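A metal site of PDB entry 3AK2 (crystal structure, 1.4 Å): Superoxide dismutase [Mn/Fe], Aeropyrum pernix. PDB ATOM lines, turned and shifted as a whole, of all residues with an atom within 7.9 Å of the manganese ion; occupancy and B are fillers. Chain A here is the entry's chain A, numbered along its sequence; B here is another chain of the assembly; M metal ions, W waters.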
ATOM      1  N   HIS A  31      10.692 -20.342  24.433  1.00  0.00           N
ATOM      2  CA  HIS A  31      11.243 -19.042  24.094  1.00  0.00           C
ATOM      3  C   HIS A  31      12.469 -18.736  24.946  1.00  0.00           C
ATOM      4  O   HIS A  31      13.484 -18.239  24.456  1.00  0.00           O
ATOM      5  CB  HIS A  31      10.177 -17.976  24.297  1.00  0.00           C
ATOM      6  CG  HIS A  31      10.432 -16.711  23.531  1.00  0.00           C
ATOM      7  ND1 HIS A  31       9.523 -15.673  23.503  1.00  0.00           N
ATOM      8  CD2 HIS A  31      11.471 -16.333  22.759  1.00  0.00           C
ATOM      9  CE1 HIS A  31      10.011 -14.702  22.749  1.00  0.00           C
ATOM     10  NE2 HIS A  31      11.189 -15.082  22.283  1.00  0.00           N
ATOM     11  N   HIS A  32      12.360 -19.064  26.231  1.00  0.00           N
ATOM     12  CA  HIS A  32      13.410 -18.814  27.195  1.00  0.00           C
ATOM     13  C   HIS A  32      14.519 -19.851  27.093  1.00  0.00           C
ATOM     14  O   HIS A  32      15.692 -19.501  26.931  1.00  0.00           O
ATOM     15  CB  HIS A  32      12.785 -18.815  28.591  1.00  0.00           C
ATOM     16  CG  HIS A  32      13.749 -18.514  29.694  1.00  0.00           C
ATOM     17  ND1 HIS A  32      13.970 -19.391  30.743  1.00  0.00           N
ATOM     18  CD2 HIS A  32      14.545 -17.440  29.917  1.00  0.00           C
ATOM     19  CE1 HIS A  32      14.859 -18.863  31.569  1.00  0.00           C
ATOM     20  NE2 HIS A  32      15.219 -17.684  31.092  1.00  0.00           N
ATOM     21  N   HIS A  35      15.326 -20.448  22.573  1.00  0.00           N
ATOM     22  CA  HIS A  35      15.722 -19.294  21.781  1.00  0.00           C
ATOM     23  C   HIS A  35      16.653 -18.333  22.520  1.00  0.00           C
ATOM     24  O   HIS A  35      17.756 -18.063  22.040  1.00  0.00           O
ATOM     25  CB  HIS A  35      14.497 -18.581  21.212  1.00  0.00           C
ATOM     26  CG  HIS A  35      13.677 -19.444  20.312  1.00  0.00           C
ATOM     27  ND1 HIS A  35      14.067 -19.752  19.028  1.00  0.00           N
ATOM     28  CD2 HIS A  35      12.513 -20.111  20.527  1.00  0.00           C
ATOM     29  CE1 HIS A  35      13.166 -20.548  18.477  1.00  0.00           C
ATOM     30  NE2 HIS A  35      12.217 -20.786  19.362  1.00  0.00           N
ATOM     31  N   HIS A  36      16.242 -17.826  23.669  1.00  0.00           N
ATOM     32  CA  HIS A  36      17.100 -16.881  24.371  1.00  0.00           C
ATOM     33  C   HIS A  36      18.440 -17.536  24.711  1.00  0.00           C
ATOM     34  O   HIS A  36      19.501 -16.948  24.494  1.00  0.00           O
ATOM     35  CB  HIS A  36      16.412 -16.306  25.608  1.00  0.00           C
ATOM     36  CG  HIS A  36      17.150 -15.159  26.233  1.00  0.00           C
ATOM     37  ND1 HIS A  36      16.652 -14.442  27.303  1.00  0.00           N
ATOM     38  CD2 HIS A  36      18.351 -14.600  25.935  1.00  0.00           C
ATOM     39  CE1 HIS A  36      17.521 -13.512  27.647  1.00  0.00           C
ATOM     40  NE2 HIS A  36      18.556 -13.584  26.828  1.00  0.00           N
ATOM     41  N   TYR A  39      20.914 -17.472  21.869  1.00  0.00           N
ATOM     42  CA  TYR A  39      21.571 -16.185  21.623  1.00  0.00           C
ATOM     43  C   TYR A  39      22.704 -15.939  22.620  1.00  0.00           C
ATOM     44  O   TYR A  39      23.774 -15.456  22.247  1.00  0.00           O
ATOM     45  CB  TYR A  39      20.578 -15.021  21.614  1.00  0.00           C
ATOM     46  CG  TYR A  39      19.369 -15.272  20.738  1.00  0.00           C
ATOM     47  CD1 TYR A  39      19.516 -15.718  19.422  1.00  0.00           C
ATOM     48  CD2 TYR A  39      18.088 -15.049  21.230  1.00  0.00           C
ATOM     49  CE1 TYR A  39      18.397 -15.952  18.625  1.00  0.00           C
ATOM     50  CE2 TYR A  39      16.974 -15.278  20.444  1.00  0.00           C
ATOM     51  CZ  TYR A  39      17.134 -15.728  19.159  1.00  0.00           C
ATOM     52  OH  TYR A  39      16.014 -15.932  18.389  1.00  0.00           O
ATOM     53  N   GLY A  75      20.163 -10.344  20.185  1.00  0.00           N
ATOM     54  CA  GLY A  75      19.114 -11.247  20.646  1.00  0.00           C
ATOM     55  C   GLY A  75      19.098 -11.328  22.161  1.00  0.00           C
ATOM     56  O   GLY A  75      18.042 -11.280  22.798  1.00  0.00           O
ATOM     57  N   MET A  78      17.876  -7.856  23.767  1.00  0.00           N
ATOM     58  CA  MET A  78      16.468  -7.624  23.471  1.00  0.00           C
ATOM     59  C   MET A  78      15.560  -8.529  24.308  1.00  0.00           C
ATOM     60  O   MET A  78      14.570  -8.065  24.855  1.00  0.00           O
ATOM     61  CB  MET A  78      16.154  -7.767  21.978  1.00  0.00           C
ATOM     62  CG  MET A  78      16.874  -6.754  21.079  1.00  0.00           C
ATOM     63  SD  MET A  78      16.391  -5.025  21.346  1.00  0.00           S
ATOM     64  CE  MET A  78      14.759  -5.003  20.583  1.00  0.00           C
ATOM     65  N   HIS A  79      15.916  -9.806  24.445  1.00  0.00           N
ATOM     66  CA  HIS A  79      15.121 -10.703  25.289  1.00  0.00           C
ATOM     67  C   HIS A  79      15.250 -10.355  26.774  1.00  0.00           C
ATOM     68  O   HIS A  79      14.299 -10.478  27.530  1.00  0.00           O
ATOM     69  CB  HIS A  79      15.459 -12.174  25.038  1.00  0.00           C
ATOM     70  CG  HIS A  79      14.971 -12.679  23.708  1.00  0.00           C
ATOM     71  ND1 HIS A  79      15.671 -12.456  22.534  1.00  0.00           N
ATOM     72  CD2 HIS A  79      13.866 -13.360  23.366  1.00  0.00           C
ATOM     73  CE1 HIS A  79      15.001 -12.984  21.529  1.00  0.00           C
ATOM     74  NE2 HIS A  79      13.904 -13.546  22.001  1.00  0.00           N
ATOM     75  N   PHE A  82      12.814  -7.731  27.173  1.00  0.00           N
ATOM     76  CA  PHE A  82      11.482  -8.279  26.909  1.00  0.00           C
ATOM     77  C   PHE A  82      10.815  -8.928  28.127  1.00  0.00           C
ATOM     78  O   PHE A  82       9.643  -8.659  28.407  1.00  0.00           O
ATOM     79  CB  PHE A  82      11.575  -9.267  25.739  1.00  0.00           C
ATOM     80  CG  PHE A  82      10.251  -9.835  25.280  1.00  0.00           C
ATOM     81  CD1 PHE A  82       9.218  -9.009  24.860  1.00  0.00           C
ATOM     82  CD2 PHE A  82      10.062 -11.218  25.216  1.00  0.00           C
ATOM     83  CE1 PHE A  82       7.996  -9.543  24.416  1.00  0.00           C
ATOM     84  CE2 PHE A  82       8.856 -11.766  24.780  1.00  0.00           C
ATOM     85  CZ  PHE A  82       7.826 -10.926  24.377  1.00  0.00           C
ATOM     86  N   TRP A  83      11.540  -9.778  28.851  1.00  0.00           N
ATOM     87  CA  TRP A  83      10.909 -10.505  29.954  1.00  0.00           C
ATOM     88  C   TRP A  83      10.374  -9.603  31.080  1.00  0.00           C
ATOM     89  O   TRP A  83       9.194  -9.682  31.419  1.00  0.00           O
ATOM     90  CB  TRP A  83      11.807 -11.610  30.531  1.00  0.00           C
ATOM     91  CG  TRP A  83      12.486 -12.508  29.543  1.00  0.00           C
ATOM     92  CD1 TRP A  83      13.821 -12.766  29.472  1.00  0.00           C
ATOM     93  CD2 TRP A  83      11.862 -13.300  28.516  1.00  0.00           C
ATOM     94  NE1 TRP A  83      14.071 -13.664  28.460  1.00  0.00           N
ATOM     95  CE2 TRP A  83      12.896 -14.012  27.865  1.00  0.00           C
ATOM     96  CE3 TRP A  83      10.534 -13.499  28.094  1.00  0.00           C
ATOM     97  CZ2 TRP A  83      12.653 -14.884  26.803  1.00  0.00           C
ATOM     98  CZ3 TRP A  83      10.296 -14.365  27.044  1.00  0.00           C
ATOM     99  CH2 TRP A  83      11.353 -15.049  26.412  1.00  0.00           C
ATOM    100  N   GLY A 129      11.138  -9.753  13.937  1.00  0.00           N
ATOM    101  CA  GLY A 129      11.744  -8.583  14.559  1.00  0.00           C
ATOM    102  C   GLY A 129      11.014  -8.128  15.803  1.00  0.00           C
ATOM    103  O   GLY A 129      10.413  -8.931  16.518  1.00  0.00           O
ATOM    104  N   TRP A 130      11.074  -6.820  16.043  1.00  0.00           N
ATOM    105  CA  TRP A 130      10.617  -6.218  17.292  1.00  0.00           C
ATOM    106  C   TRP A 130       9.936  -4.893  17.030  1.00  0.00           C
ATOM    107  O   TRP A 130      10.321  -4.156  16.138  1.00  0.00           O
ATOM    108  CB  TRP A 130      11.825  -5.927  18.202  1.00  0.00           C
ATOM    109  CG  TRP A 130      12.647  -7.119  18.507  1.00  0.00           C
ATOM    110  CD1 TRP A 130      13.598  -7.691  17.718  1.00  0.00           C
ATOM    111  CD2 TRP A 130      12.609  -7.896  19.714  1.00  0.00           C
ATOM    112  NE1 TRP A 130      14.143  -8.781  18.348  1.00  0.00           N
ATOM    113  CE2 TRP A 130      13.557  -8.928  19.571  1.00  0.00           C
ATOM    114  CE3 TRP A 130      11.867  -7.827  20.902  1.00  0.00           C
ATOM    115  CZ2 TRP A 130      13.788  -9.887  20.561  1.00  0.00           C
ATOM    116  CZ3 TRP A 130      12.096  -8.761  21.890  1.00  0.00           C
ATOM    117  CH2 TRP A 130      13.038  -9.784  21.711  1.00  0.00           C
ATOM    118  N   HIS A 150      17.351  -9.137  15.075  1.00  0.00           N
ATOM    119  CA  HIS A 150      17.626  -8.446  16.342  1.00  0.00           C
ATOM    120  C   HIS A 150      18.457  -7.198  16.141  1.00  0.00           C
ATOM    121  O   HIS A 150      18.626  -6.412  17.066  1.00  0.00           O
ATOM    122  CB  HIS A 150      18.388  -9.363  17.284  1.00  0.00           C
ATOM    123  CG  HIS A 150      17.652 -10.610  17.612  1.00  0.00           C
ATOM    124  ND1 HIS A 150      18.203 -11.868  17.513  1.00  0.00           N
ATOM    125  CD2 HIS A 150      16.378 -10.794  18.034  1.00  0.00           C
ATOM    126  CE1 HIS A 150      17.302 -12.765  17.857  1.00  0.00           C
ATOM    127  NE2 HIS A 150      16.191 -12.138  18.178  1.00  0.00           N
ATOM    128  N   ILE A 164       8.410  -5.351  22.074  1.00  0.00           N
ATOM    129  CA  ILE A 164       7.572  -6.523  21.823  1.00  0.00           C
ATOM    130  C   ILE A 164       8.245  -7.380  20.768  1.00  0.00           C
ATOM    131  O   ILE A 164       8.620  -6.901  19.690  1.00  0.00           O
ATOM    132  CB  ILE A 164       6.114  -6.164  21.422  1.00  0.00           C
ATOM    133  CG1 ILE A 164       5.283  -7.452  21.264  1.00  0.00           C
ATOM    134  CG2 ILE A 164       6.076  -5.310  20.162  1.00  0.00           C
ATOM    135  CD1 ILE A 164       3.827  -7.248  20.842  1.00  0.00           C
ATOM    136  N   ASP A 165       8.398  -8.664  21.080  1.00  0.00           N
ATOM    137  CA  ASP A 165       8.978  -9.635  20.178  1.00  0.00           C
ATOM    138  C   ASP A 165       7.900 -10.087  19.204  1.00  0.00           C
ATOM    139  O   ASP A 165       6.869 -10.631  19.631  1.00  0.00           O
ATOM    140  CB  ASP A 165       9.489 -10.817  20.984  1.00  0.00           C
ATOM    141  CG  ASP A 165      10.336 -11.775  20.186  1.00  0.00           C
ATOM    142  OD1 ASP A 165      10.523 -11.586  18.958  1.00  0.00           O
ATOM    143  OD2 ASP A 165      10.828 -12.729  20.809  1.00  0.00           O
ATOM    144  N   VAL A 166       8.108  -9.854  17.912  1.00  0.00           N
ATOM    145  CA  VAL A 166       7.211 -10.380  16.887  1.00  0.00           C
ATOM    146  C   VAL A 166       7.891 -11.385  15.957  1.00  0.00           C
ATOM    147  O   VAL A 166       7.423 -11.622  14.836  1.00  0.00           O
ATOM    148  CB  VAL A 166       6.458  -9.275  16.087  1.00  0.00           C
ATOM    149  CG1 VAL A 166       5.454  -8.557  16.991  1.00  0.00           C
ATOM    150  CG2 VAL A 166       7.426  -8.286  15.461  1.00  0.00           C
ATOM    151  N   TRP A 167       8.976 -12.003  16.424  1.00  0.00           N
ATOM    152  CA  TRP A 167       9.434 -13.220  15.783  1.00  0.00           C
ATOM    153  C   TRP A 167       8.297 -14.228  15.845  1.00  0.00           C
ATOM    154  O   TRP A 167       7.510 -14.219  16.787  1.00  0.00           O
ATOM    155  CB  TRP A 167      10.639 -13.801  16.500  1.00  0.00           C
ATOM    156  CG  TRP A 167      11.947 -13.117  16.190  1.00  0.00           C
ATOM    157  CD1 TRP A 167      12.259 -11.806  16.410  1.00  0.00           C
ATOM    158  CD2 TRP A 167      13.102 -13.726  15.623  1.00  0.00           C
ATOM    159  NE1 TRP A 167      13.550 -11.560  16.011  1.00  0.00           N
ATOM    160  CE2 TRP A 167      14.091 -12.718  15.533  1.00  0.00           C
ATOM    161  CE3 TRP A 167      13.412 -15.018  15.191  1.00  0.00           C
ATOM    162  CZ2 TRP A 167      15.364 -12.970  15.007  1.00  0.00           C
ATOM    163  CZ3 TRP A 167      14.670 -15.263  14.668  1.00  0.00           C
ATOM    164  CH2 TRP A 167      15.641 -14.241  14.587  1.00  0.00           C
ATOM    165  N   GLU A 168       8.212 -15.095  14.846  1.00  0.00           N
ATOM    166  CA  GLU A 168       7.116 -16.052  14.799  1.00  0.00           C
ATOM    167  C   GLU A 168       7.095 -16.967  16.020  1.00  0.00           C
ATOM    168  O   GLU A 168       6.026 -17.296  16.530  1.00  0.00           O
ATOM    169  CB  GLU A 168       7.131 -16.833  13.481  1.00  0.00           C
ATOM    170  CG  GLU A 168       6.885 -15.923  12.277  1.00  0.00           C
ATOM    171  CD  GLU A 168       6.899 -16.635  10.944  1.00  0.00           C
ATOM    172  OE1 GLU A 168       7.767 -17.505  10.725  1.00  0.00           O
ATOM    173  OE2 GLU A 168       6.042 -16.298  10.098  1.00  0.00           O
ATOM    174  N   HIS A 169       8.279 -17.334  16.520  1.00  0.00           N
ATOM    175  CA  HIS A 169       8.353 -18.188  17.714  1.00  0.00           C
ATOM    176  C   HIS A 169       7.731 -17.579  18.956  1.00  0.00           C
ATOM    177  O   HIS A 169       7.457 -18.293  19.924  1.00  0.00           O
ATOM    178  CB  HIS A 169       9.793 -18.647  18.002  1.00  0.00           C
ATOM    179  CG  HIS A 169      10.731 -17.539  18.408  1.00  0.00           C
ATOM    180  ND1 HIS A 169      11.846 -17.215  17.670  1.00  0.00           N
ATOM    181  CD2 HIS A 169      10.758 -16.723  19.490  1.00  0.00           C
ATOM    182  CE1 HIS A 169      12.502 -16.234  18.267  1.00  0.00           C
ATOM    183  NE2 HIS A 169      11.856 -15.914  19.371  1.00  0.00           N
ATOM    184  N   ALA A 170       7.526 -16.265  18.963  1.00  0.00           N
ATOM    185  CA  ALA A 170       6.920 -15.594  20.110  1.00  0.00           C
ATOM    186  C   ALA A 170       5.405 -15.812  20.199  1.00  0.00           C
ATOM    187  O   ALA A 170       4.813 -15.584  21.255  1.00  0.00           O
ATOM    188  CB  ALA A 170       7.252 -14.095  20.091  1.00  0.00           C
ATOM    189  N   TYR A 182      -2.055 -11.517  18.563  1.00  0.00           N
ATOM    190  CA  TYR A 182      -0.984 -11.589  19.552  1.00  0.00           C
ATOM    191  C   TYR A 182      -0.609 -10.210  20.108  1.00  0.00           C
ATOM    192  O   TYR A 182      -0.537 -10.031  21.328  1.00  0.00           O
ATOM    193  CB  TYR A 182       0.255 -12.278  18.970  1.00  0.00           C
ATOM    194  CG  TYR A 182       1.550 -12.024  19.716  1.00  0.00           C
ATOM    195  CD1 TYR A 182       1.742 -12.506  21.002  1.00  0.00           C
ATOM    196  CD2 TYR A 182       2.587 -11.339  19.102  1.00  0.00           C
ATOM    197  CE1 TYR A 182       2.941 -12.289  21.681  1.00  0.00           C
ATOM    198  CE2 TYR A 182       3.800 -11.113  19.771  1.00  0.00           C
ATOM    199  CZ  TYR A 182       3.964 -11.598  21.054  1.00  0.00           C
ATOM    200  OH  TYR A 182       5.144 -11.397  21.732  1.00  0.00           O
ATOM    201  N   GLU B 168      10.140 -19.713  10.442  1.00  0.00           N
ATOM    202  CA  GLU B 168       9.611 -20.465  11.581  1.00  0.00           C
ATOM    203  C   GLU B 168       8.230 -21.054  11.291  1.00  0.00           C
ATOM    204  O   GLU B 168       7.943 -22.187  11.698  1.00  0.00           O
ATOM    205  CB  GLU B 168       9.646 -19.598  12.854  1.00  0.00           C
ATOM    206  CG  GLU B 168      11.077 -19.250  13.261  1.00  0.00           C
ATOM    207  CD  GLU B 168      11.172 -18.362  14.481  1.00  0.00           C
ATOM    208  OE1 GLU B 168      10.361 -17.424  14.609  1.00  0.00           O
ATOM    209  OE2 GLU B 168      12.084 -18.615  15.305  1.00  0.00           O
HETATM  210 MN    MN M   1      12.283 -14.138  20.632  1.00  0.00          MN
HETATM  211  O   HOH W   1      13.097 -13.017  19.028  1.00  0.00           O
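N of Trp 167 lies within hydrogen-bond range of OD1 of Asp 165, 3.0 Å away.
A ring nitrogen (ND1) of His 79 is in hydrogen-bond range of the backbone carbonyl oxygen (O) of Gly 75.
OE2 of Glu 168 of chain B lies within hydrogen-bond range of ND1 of His 169 (2.8 Å).
The backbone carbonyl oxygen (O) of His 31 lies within hydrogen-bond range of the backbone NH (N) of His 36.
The backbone carbonyl oxygen of His 79 sits close to the indole nitrogen of Trp 83.
O of Asp 165 is in hydrogen-bond range of OH of Tyr 182, at 2.8 Å.
Within 4 Å of the manganese ion: His 31, His 79, Asp 165 and His 169.
The manganese ion is bound by the side-chain carboxylate of Asp 165 (2.0 Å), water W1 (2.1 Å), a ring nitrogen (NE2) of His 31 (2.2 Å), a ring nitrogen (NE2) of His 79 (2.2 Å) and a ring nitrogen (NE2) of His 169 (2.2 Å).
Water W1 lies within hydrogen-bond range of the side-chain carboxylate (OD1) of Asp 165, a ring nitrogen (NE2) of His 150 and the indole nitrogen (NE1) of Trp 167.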
